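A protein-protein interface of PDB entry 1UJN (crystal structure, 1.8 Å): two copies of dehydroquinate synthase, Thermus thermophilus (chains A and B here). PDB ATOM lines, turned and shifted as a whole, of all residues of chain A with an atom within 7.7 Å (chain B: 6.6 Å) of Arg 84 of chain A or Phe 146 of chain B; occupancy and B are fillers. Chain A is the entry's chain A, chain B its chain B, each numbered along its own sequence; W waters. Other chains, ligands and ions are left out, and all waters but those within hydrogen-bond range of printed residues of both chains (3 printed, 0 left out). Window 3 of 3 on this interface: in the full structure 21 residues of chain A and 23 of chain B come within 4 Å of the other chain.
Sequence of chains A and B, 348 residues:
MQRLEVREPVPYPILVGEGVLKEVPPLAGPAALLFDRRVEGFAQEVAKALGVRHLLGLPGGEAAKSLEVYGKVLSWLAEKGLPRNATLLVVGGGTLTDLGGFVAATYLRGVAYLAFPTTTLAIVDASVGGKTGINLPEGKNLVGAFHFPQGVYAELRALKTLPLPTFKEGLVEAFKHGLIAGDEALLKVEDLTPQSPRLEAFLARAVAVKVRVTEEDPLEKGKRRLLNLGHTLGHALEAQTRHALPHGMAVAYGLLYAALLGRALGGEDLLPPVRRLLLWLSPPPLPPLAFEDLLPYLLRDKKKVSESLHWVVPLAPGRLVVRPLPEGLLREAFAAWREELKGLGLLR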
ATOM      1  N   PRO A  30       8.827   4.364 -32.451  1.00  0.00           N
ATOM      2  CA  PRO A  30       7.958   5.351 -33.097  1.00  0.00           C
ATOM      3  C   PRO A  30       8.413   6.778 -32.792  1.00  0.00           C
ATOM      4  O   PRO A  30       9.212   7.002 -31.873  1.00  0.00           O
ATOM      5  CB  PRO A  30       6.574   5.027 -32.529  1.00  0.00           C
ATOM      6  CG  PRO A  30       6.632   3.648 -31.941  1.00  0.00           C
ATOM      7  CD  PRO A  30       8.070   3.527 -31.505  1.00  0.00           C
ATOM      8  N   GLY A  81      -1.704   7.480 -31.065  1.00  0.00           N
ATOM      9  CA  GLY A  81      -1.401   6.280 -30.313  1.00  0.00           C
ATOM     10  C   GLY A  81       0.078   6.066 -30.044  1.00  0.00           C
ATOM     11  O   GLY A  81       0.517   4.933 -29.878  1.00  0.00           O
ATOM     12  N   LEU A  82       0.851   7.145 -29.996  1.00  0.00           N
ATOM     13  CA  LEU A  82       2.285   7.014 -29.738  1.00  0.00           C
ATOM     14  C   LEU A  82       2.539   6.416 -28.360  1.00  0.00           C
ATOM     15  O   LEU A  82       2.026   6.908 -27.356  1.00  0.00           O
ATOM     16  CB  LEU A  82       2.987   8.368 -29.857  1.00  0.00           C
ATOM     17  CG  LEU A  82       3.239   8.838 -31.294  1.00  0.00           C
ATOM     18  CD1 LEU A  82       3.869  10.216 -31.281  1.00  0.00           C
ATOM     19  CD2 LEU A  82       4.151   7.846 -32.002  1.00  0.00           C
ATOM     20  N   PRO A  83       3.335   5.333 -28.299  1.00  0.00           N
ATOM     21  CA  PRO A  83       3.675   4.639 -27.057  1.00  0.00           C
ATOM     22  C   PRO A  83       4.811   5.274 -26.260  1.00  0.00           C
ATOM     23  O   PRO A  83       5.435   6.241 -26.697  1.00  0.00           O
ATOM     24  CB  PRO A  83       4.009   3.231 -27.538  1.00  0.00           C
ATOM     25  CG  PRO A  83       4.665   3.493 -28.849  1.00  0.00           C
ATOM     26  CD  PRO A  83       3.804   4.567 -29.471  1.00  0.00           C
ATOM     27  N   ARG A  84       5.077   4.702 -25.091  1.00  0.00           N
ATOM     28  CA  ARG A  84       6.096   5.202 -24.157  1.00  0.00           C
ATOM     29  C   ARG A  84       7.527   5.138 -24.727  1.00  0.00           C
ATOM     30  O   ARG A  84       8.437   5.817 -24.269  1.00  0.00           O
ATOM     31  CB  ARG A  84       6.010   4.379 -22.871  1.00  0.00           C
ATOM     32  CG  ARG A  84       6.488   5.162 -21.649  1.00  0.00           C
ATOM     33  CD  ARG A  84       6.297   4.374 -20.348  1.00  0.00           C
ATOM     34  NE  ARG A  84       7.403   4.637 -19.420  1.00  0.00           N
ATOM     35  CZ  ARG A  84       7.194   4.366 -18.119  1.00  0.00           C
ATOM     36  NH1 ARG A  84       6.034   3.878 -17.718  1.00  0.00           N
ATOM     37  NH2 ARG A  84       8.171   4.587 -17.234  1.00  0.00           N
ATOM     38  N   ASN A  85       7.768   4.305 -25.736  1.00  0.00           N
ATOM     39  CA  ASN A  85       9.114   4.221 -26.299  1.00  0.00           C
ATOM     40  C   ASN A  85       9.254   5.143 -27.506  1.00  0.00           C
ATOM     41  O   ASN A  85      10.223   5.055 -28.264  1.00  0.00           O
ATOM     42  CB  ASN A  85       9.462   2.774 -26.683  1.00  0.00           C
ATOM     43  CG  ASN A  85       8.631   2.250 -27.836  1.00  0.00           C
ATOM     44  OD1 ASN A  85       7.423   2.468 -27.896  1.00  0.00           O
ATOM     45  ND2 ASN A  85       9.277   1.534 -28.750  1.00  0.00           N
ATOM     46  N   ALA A  86       8.289   6.041 -27.675  1.00  0.00           N
ATOM     47  CA  ALA A  86       8.329   6.990 -28.781  1.00  0.00           C
ATOM     48  C   ALA A  86       9.320   8.118 -28.481  1.00  0.00           C
ATOM     49  O   ALA A  86       9.685   8.364 -27.324  1.00  0.00           O
ATOM     50  CB  ALA A  86       6.936   7.576 -29.028  1.00  0.00           C
ATOM     51  N   THR A  87       9.753   8.794 -29.535  1.00  0.00           N
ATOM     52  CA  THR A  87      10.674   9.916 -29.406  1.00  0.00           C
ATOM     53  C   THR A  87      10.030  11.139 -30.037  1.00  0.00           C
ATOM     54  O   THR A  87       9.481  11.061 -31.139  1.00  0.00           O
ATOM     55  CB  THR A  87      12.005   9.656 -30.144  1.00  0.00           C
ATOM     56  OG1 THR A  87      12.647   8.505 -29.587  1.00  0.00           O
ATOM     57  CG2 THR A  87      12.937  10.863 -30.011  1.00  0.00           C
ATOM     58  N   ALA A 105       8.310  15.574 -21.384  1.00  0.00           N
ATOM     59  CA  ALA A 105       8.486  15.256 -19.975  1.00  0.00           C
ATOM     60  C   ALA A 105       7.239  14.694 -19.316  1.00  0.00           C
ATOM     61  O   ALA A 105       7.342  13.958 -18.337  1.00  0.00           O
ATOM     62  CB  ALA A 105       8.943  16.498 -19.208  1.00  0.00           C
ATOM     63  N   TYR A 107       4.118  13.506 -21.313  1.00  0.00           N
ATOM     64  CA  TYR A 107       3.301  12.586 -22.101  1.00  0.00           C
ATOM     65  C   TYR A 107       3.630  11.180 -21.595  1.00  0.00           C
ATOM     66  O   TYR A 107       4.794  10.775 -21.609  1.00  0.00           O
ATOM     67  CB  TYR A 107       3.639  12.702 -23.595  1.00  0.00           C
ATOM     68  CG  TYR A 107       2.830  11.759 -24.472  1.00  0.00           C
ATOM     69  CD1 TYR A 107       1.445  11.876 -24.558  1.00  0.00           C
ATOM     70  CD2 TYR A 107       3.449  10.727 -25.181  1.00  0.00           C
ATOM     71  CE1 TYR A 107       0.689  10.988 -25.326  1.00  0.00           C
ATOM     72  CE2 TYR A 107       2.701   9.830 -25.954  1.00  0.00           C
ATOM     73  CZ  TYR A 107       1.321   9.970 -26.017  1.00  0.00           C
ATOM     74  OH  TYR A 107       0.567   9.092 -26.769  1.00  0.00           O
ATOM     75  N   LEU A 108       2.608  10.452 -21.142  1.00  0.00           N
ATOM     76  CA  LEU A 108       2.777   9.101 -20.596  1.00  0.00           C
ATOM     77  C   LEU A 108       3.818   9.096 -19.473  1.00  0.00           C
ATOM     78  O   LEU A 108       4.483   8.096 -19.219  1.00  0.00           O
ATOM     79  CB  LEU A 108       3.182   8.121 -21.704  1.00  0.00           C
ATOM     80  CG  LEU A 108       2.187   8.006 -22.865  1.00  0.00           C
ATOM     81  CD1 LEU A 108       2.714   7.036 -23.910  1.00  0.00           C
ATOM     82  CD2 LEU A 108       0.833   7.552 -22.335  1.00  0.00           C
ATOM     83  N   ARG A 109       3.926  10.234 -18.798  1.00  0.00           N
ATOM     84  CA  ARG A 109       4.851  10.457 -17.696  1.00  0.00           C
ATOM     85  C   ARG A 109       6.306  10.550 -18.146  1.00  0.00           C
ATOM     86  O   ARG A 109       7.225  10.398 -17.340  1.00  0.00           O
ATOM     87  CB  ARG A 109       4.695   9.388 -16.595  1.00  0.00           C
ATOM     88  CG  ARG A 109       3.271   9.271 -16.050  1.00  0.00           C
ATOM     89  CD  ARG A 109       3.239   8.600 -14.679  1.00  0.00           C
ATOM     90  NE  ARG A 109       1.874   8.415 -14.195  1.00  0.00           N
ATOM     91  CZ  ARG A 109       1.128   7.342 -14.439  1.00  0.00           C
ATOM     92  NH1 ARG A 109       1.613   6.340 -15.168  1.00  0.00           N
ATOM     93  NH2 ARG A 109      -0.105   7.268 -13.948  1.00  0.00           N
ATOM     94  N   GLY A 110       6.512  10.799 -19.435  1.00  0.00           N
ATOM     95  CA  GLY A 110       7.865  10.972 -19.922  1.00  0.00           C
ATOM     96  C   GLY A 110       8.360  10.110 -21.060  1.00  0.00           C
ATOM     97  O   GLY A 110       8.412   8.890 -20.948  1.00  0.00           O
ATOM     98  N   VAL A 111       8.731  10.766 -22.158  1.00  0.00           N
ATOM     99  CA  VAL A 111       9.287  10.092 -23.321  1.00  0.00           C
ATOM    100  C   VAL A 111      10.531  10.865 -23.748  1.00  0.00           C
ATOM    101  O   VAL A 111      10.717  12.029 -23.383  1.00  0.00           O
ATOM    102  CB  VAL A 111       8.298  10.040 -24.509  1.00  0.00           C
ATOM    103  CG1 VAL A 111       7.053   9.234 -24.115  1.00  0.00           C
ATOM    104  CG2 VAL A 111       7.916  11.461 -24.945  1.00  0.00           C
ATOM    105  N   ALA A 112      11.387  10.215 -24.518  1.00  0.00           N
ATOM    106  CA  ALA A 112      12.612  10.857 -24.981  1.00  0.00           C
ATOM    107  C   ALA A 112      12.325  11.939 -26.012  1.00  0.00           C
ATOM    108  O   ALA A 112      11.312  11.893 -26.715  1.00  0.00           O
ATOM    109  CB  ALA A 112      13.537   9.807 -25.589  1.00  0.00           C
ATOM    110  N   ALA B 105       4.287  18.232  -9.087  1.00  0.00           N
ATOM    111  CA  ALA B 105       5.426  17.849  -9.915  1.00  0.00           C
ATOM    112  C   ALA B 105       5.816  18.897 -10.953  1.00  0.00           C
ATOM    113  O   ALA B 105       6.977  18.967 -11.365  1.00  0.00           O
ATOM    114  CB  ALA B 105       5.132  16.516 -10.618  1.00  0.00           C
ATOM    115  N   GLY B 129       4.902   4.271  -5.309  1.00  0.00           N
ATOM    116  CA  GLY B 129       5.000   4.329  -6.762  1.00  0.00           C
ATOM    117  C   GLY B 129       5.190   5.696  -7.402  1.00  0.00           C
ATOM    118  O   GLY B 129       5.689   5.785  -8.528  1.00  0.00           O
ATOM    119  N   GLY B 130       4.773   6.749  -6.708  1.00  0.00           N
ATOM    120  CA  GLY B 130       4.926   8.105  -7.224  1.00  0.00           C
ATOM    121  C   GLY B 130       4.164   8.400  -8.506  1.00  0.00           C
ATOM    122  O   GLY B 130       4.480   9.358  -9.217  1.00  0.00           O
ATOM    123  N   LYS B 131       3.163   7.586  -8.820  1.00  0.00           N
ATOM    124  CA  LYS B 131       2.385   7.805 -10.039  1.00  0.00           C
ATOM    125  C   LYS B 131       1.416   8.970  -9.885  1.00  0.00           C
ATOM    126  O   LYS B 131       0.562   8.951  -9.000  1.00  0.00           O
ATOM    127  CB  LYS B 131       1.582   6.553 -10.407  1.00  0.00           C
ATOM    128  CG  LYS B 131       2.391   5.411 -10.984  1.00  0.00           C
ATOM    129  CD  LYS B 131       1.468   4.339 -11.566  1.00  0.00           C
ATOM    130  CE  LYS B 131       2.260   3.214 -12.214  1.00  0.00           C
ATOM    131  NZ  LYS B 131       1.365   2.201 -12.857  1.00  0.00           N
ATOM    132  N   THR B 132       1.561   9.989 -10.733  1.00  0.00           N
ATOM    133  CA  THR B 132       0.656  11.139 -10.710  1.00  0.00           C
ATOM    134  C   THR B 132       0.255  11.428 -12.145  1.00  0.00           C
ATOM    135  O   THR B 132       0.917  10.969 -13.082  1.00  0.00           O
ATOM    136  CB  THR B 132       1.312  12.424 -10.118  1.00  0.00           C
ATOM    137  OG1 THR B 132       2.218  12.998 -11.072  1.00  0.00           O
ATOM    138  CG2 THR B 132       2.076  12.095  -8.843  1.00  0.00           C
ATOM    139  N   GLY B 144       1.313  12.893 -17.209  1.00  0.00           N
ATOM    140  CA  GLY B 144       1.636  12.839 -15.793  1.00  0.00           C
ATOM    141  C   GLY B 144       3.111  12.893 -15.479  1.00  0.00           C
ATOM    142  O   GLY B 144       3.904  13.355 -16.287  1.00  0.00           O
ATOM    143  N   ALA B 145       3.474  12.415 -14.296  1.00  0.00           N
ATOM    144  CA  ALA B 145       4.868  12.415 -13.880  1.00  0.00           C
ATOM    145  C   ALA B 145       5.072  11.503 -12.696  1.00  0.00           C
ATOM    146  O   ALA B 145       4.142  11.221 -11.938  1.00  0.00           O
ATOM    147  CB  ALA B 145       5.298  13.830 -13.503  1.00  0.00           C
ATOM    148  N   PHE B 146       6.293  11.014 -12.544  1.00  0.00           N
ATOM    149  CA  PHE B 146       6.591  10.216 -11.371  1.00  0.00           C
ATOM    150  C   PHE B 146       7.137  11.270 -10.417  1.00  0.00           C
ATOM    151  O   PHE B 146       8.173  11.893 -10.681  1.00  0.00           O
ATOM    152  CB  PHE B 146       7.633   9.142 -11.676  1.00  0.00           C
ATOM    153  CG  PHE B 146       7.090   8.000 -12.477  1.00  0.00           C
ATOM    154  CD1 PHE B 146       7.229   7.969 -13.860  1.00  0.00           C
ATOM    155  CD2 PHE B 146       6.400   6.973 -11.849  1.00  0.00           C
ATOM    156  CE1 PHE B 146       6.688   6.928 -14.606  1.00  0.00           C
ATOM    157  CE2 PHE B 146       5.850   5.924 -12.588  1.00  0.00           C
ATOM    158  CZ  PHE B 146       5.996   5.903 -13.969  1.00  0.00           C
ATOM    159  N   HIS B 147       6.409  11.497  -9.330  1.00  0.00           N
ATOM    160  CA  HIS B 147       6.789  12.495  -8.341  1.00  0.00           C
ATOM    161  C   HIS B 147       6.316  11.919  -7.016  1.00  0.00           C
ATOM    162  O   HIS B 147       5.115  11.726  -6.796  1.00  0.00           O
ATOM    163  CB  HIS B 147       6.086  13.819  -8.654  1.00  0.00           C
ATOM    164  CG  HIS B 147       6.526  14.966  -7.793  1.00  0.00           C
ATOM    165  ND1 HIS B 147       7.854  15.270  -7.575  1.00  0.00           N
ATOM    166  CD2 HIS B 147       5.812  15.908  -7.132  1.00  0.00           C
ATOM    167  CE1 HIS B 147       7.938  16.349  -6.815  1.00  0.00           C
ATOM    168  NE2 HIS B 147       6.712  16.755  -6.532  1.00  0.00           N
ATOM    169  N   PHE B 148       7.276  11.618  -6.155  1.00  0.00           N
ATOM    170  CA  PHE B 148       6.991  11.004  -4.873  1.00  0.00           C
ATOM    171  C   PHE B 148       6.648  11.992  -3.788  1.00  0.00           C
ATOM    172  O   PHE B 148       7.222  13.073  -3.714  1.00  0.00           O
ATOM    173  CB  PHE B 148       8.185  10.157  -4.429  1.00  0.00           C
ATOM    174  CG  PHE B 148       8.566   9.097  -5.420  1.00  0.00           C
ATOM    175  CD1 PHE B 148       9.470   9.371  -6.441  1.00  0.00           C
ATOM    176  CD2 PHE B 148       7.977   7.838  -5.362  1.00  0.00           C
ATOM    177  CE1 PHE B 148       9.783   8.400  -7.402  1.00  0.00           C
ATOM    178  CE2 PHE B 148       8.280   6.857  -6.314  1.00  0.00           C
ATOM    179  CZ  PHE B 148       9.186   7.143  -7.336  1.00  0.00           C
ATOM    180  N   GLU B 220      11.073  -2.838 -12.927  1.00  0.00           N
ATOM    181  CA  GLU B 220       9.914  -3.689 -13.173  1.00  0.00           C
ATOM    182  C   GLU B 220      10.219  -4.788 -14.193  1.00  0.00           C
ATOM    183  O   GLU B 220       9.554  -4.907 -15.222  1.00  0.00           O
ATOM    184  CB  GLU B 220       8.725  -2.848 -13.649  1.00  0.00           C
ATOM    185  CG  GLU B 220       7.419  -3.629 -13.718  1.00  0.00           C
ATOM    186  CD  GLU B 220       6.222  -2.757 -14.040  1.00  0.00           C
ATOM    187  OE1 GLU B 220       5.108  -3.305 -14.174  1.00  0.00           O
ATOM    188  OE2 GLU B 220       6.392  -1.524 -14.157  1.00  0.00           O
ATOM    189  N   ARG B 224       7.892  -6.733  -9.505  1.00  0.00           N
ATOM    190  CA  ARG B 224       7.031  -5.566  -9.665  1.00  0.00           C
ATOM    191  C   ARG B 224       5.864  -5.743 -10.633  1.00  0.00           C
ATOM    192  O   ARG B 224       4.797  -5.162 -10.434  1.00  0.00           O
ATOM    193  CB  ARG B 224       7.865  -4.353 -10.076  1.00  0.00           C
ATOM    194  CG  ARG B 224       7.114  -3.035 -10.011  1.00  0.00           C
ATOM    195  CD  ARG B 224       8.085  -1.865 -10.080  1.00  0.00           C
ATOM    196  NE  ARG B 224       7.427  -0.579  -9.880  1.00  0.00           N
ATOM    197  CZ  ARG B 224       8.073   0.578  -9.768  1.00  0.00           C
ATOM    198  NH1 ARG B 224       9.396   0.609  -9.837  1.00  0.00           N
ATOM    199  NH2 ARG B 224       7.398   1.704  -9.583  1.00  0.00           N
HETATM  200  O   HOH W   1      -1.498   8.719 -11.769  1.00  0.00           O
HETATM  201  O   HOH W   2       8.039  11.439 -14.711  1.00  0.00           O
HETATM  202  O   HOH W   3       6.812  13.917 -15.908  1.00  0.00           O
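OG1 of Thr 132 of chain B sits at hydrogen-bond distance from O of Ala 145 of chain B, at 2.8 Å.
Hydrophobic or aromatic side chains of chain B that line the printed part of chain A: Phe 146.
Along chain B the printed residues that touch a printed residue of chain A span positions 131 to 146.
The guanidinium group (NE) of Arg 109 of chain A lies within hydrogen-bond range of the backbone carbonyl oxygen (O) of Thr 132 of chain B, 2.9 Å away.
Water W3 bridges the backbone carbonyl oxygen of Ala 105 of chain A (2.5 Å) and the backbone carbonyl oxygen of Gly 144 of chain B (3.0 Å).
Water W2 lies within hydrogen-bond range of the backbone NH of Phe 146 of chain B (2.8 Å) and the backbone carbonyl oxygen of Arg 109 of chain A (2.9 Å).
Water W1 lies within hydrogen-bond range of the guanidinium group of Arg 109 of chain A (3.0 Å), the backbone carbonyl oxygen of Lys 131 of chain B (3.5 Å) and the backbone NH of Thr 132 of chain B (3.5 Å).
Of the printed residues of chain B, Arg 84 of chain A touches Phe 146.
Of chain A, only Arg 109 comes within 4 Å of Ala 145 of chain B.
Of the printed residues of chain A, Gly 144 of chain B touches Arg 109 (3.4 Å).
Of the printed residues of chain A, Lys 131 of chain B touches Arg 109.
Of the printed residues of chain A, Thr 132 of chain B touches Arg 109.
The nearest printed residue of chain A that does not touch Lys 131 of chain B is Arg 84 of chain A (6.7 Å).
1 position is printed for both chains.
Of the 6 pairs that touch across the chains among the printed residues, none has its exchanged pair printed and touching as well.
Among the printed residues, pairs that only touch across the chains: Arg 109 of chain A with Gly 144 of chain B, Arg 109 of chain A with Ala 145 of chain B, Arg 109 of chain A with Phe 146 of chain B, Arg 84 of chain A with Phe 146 of chain B and Arg 109 of chain A with Lys 131 of chain B.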
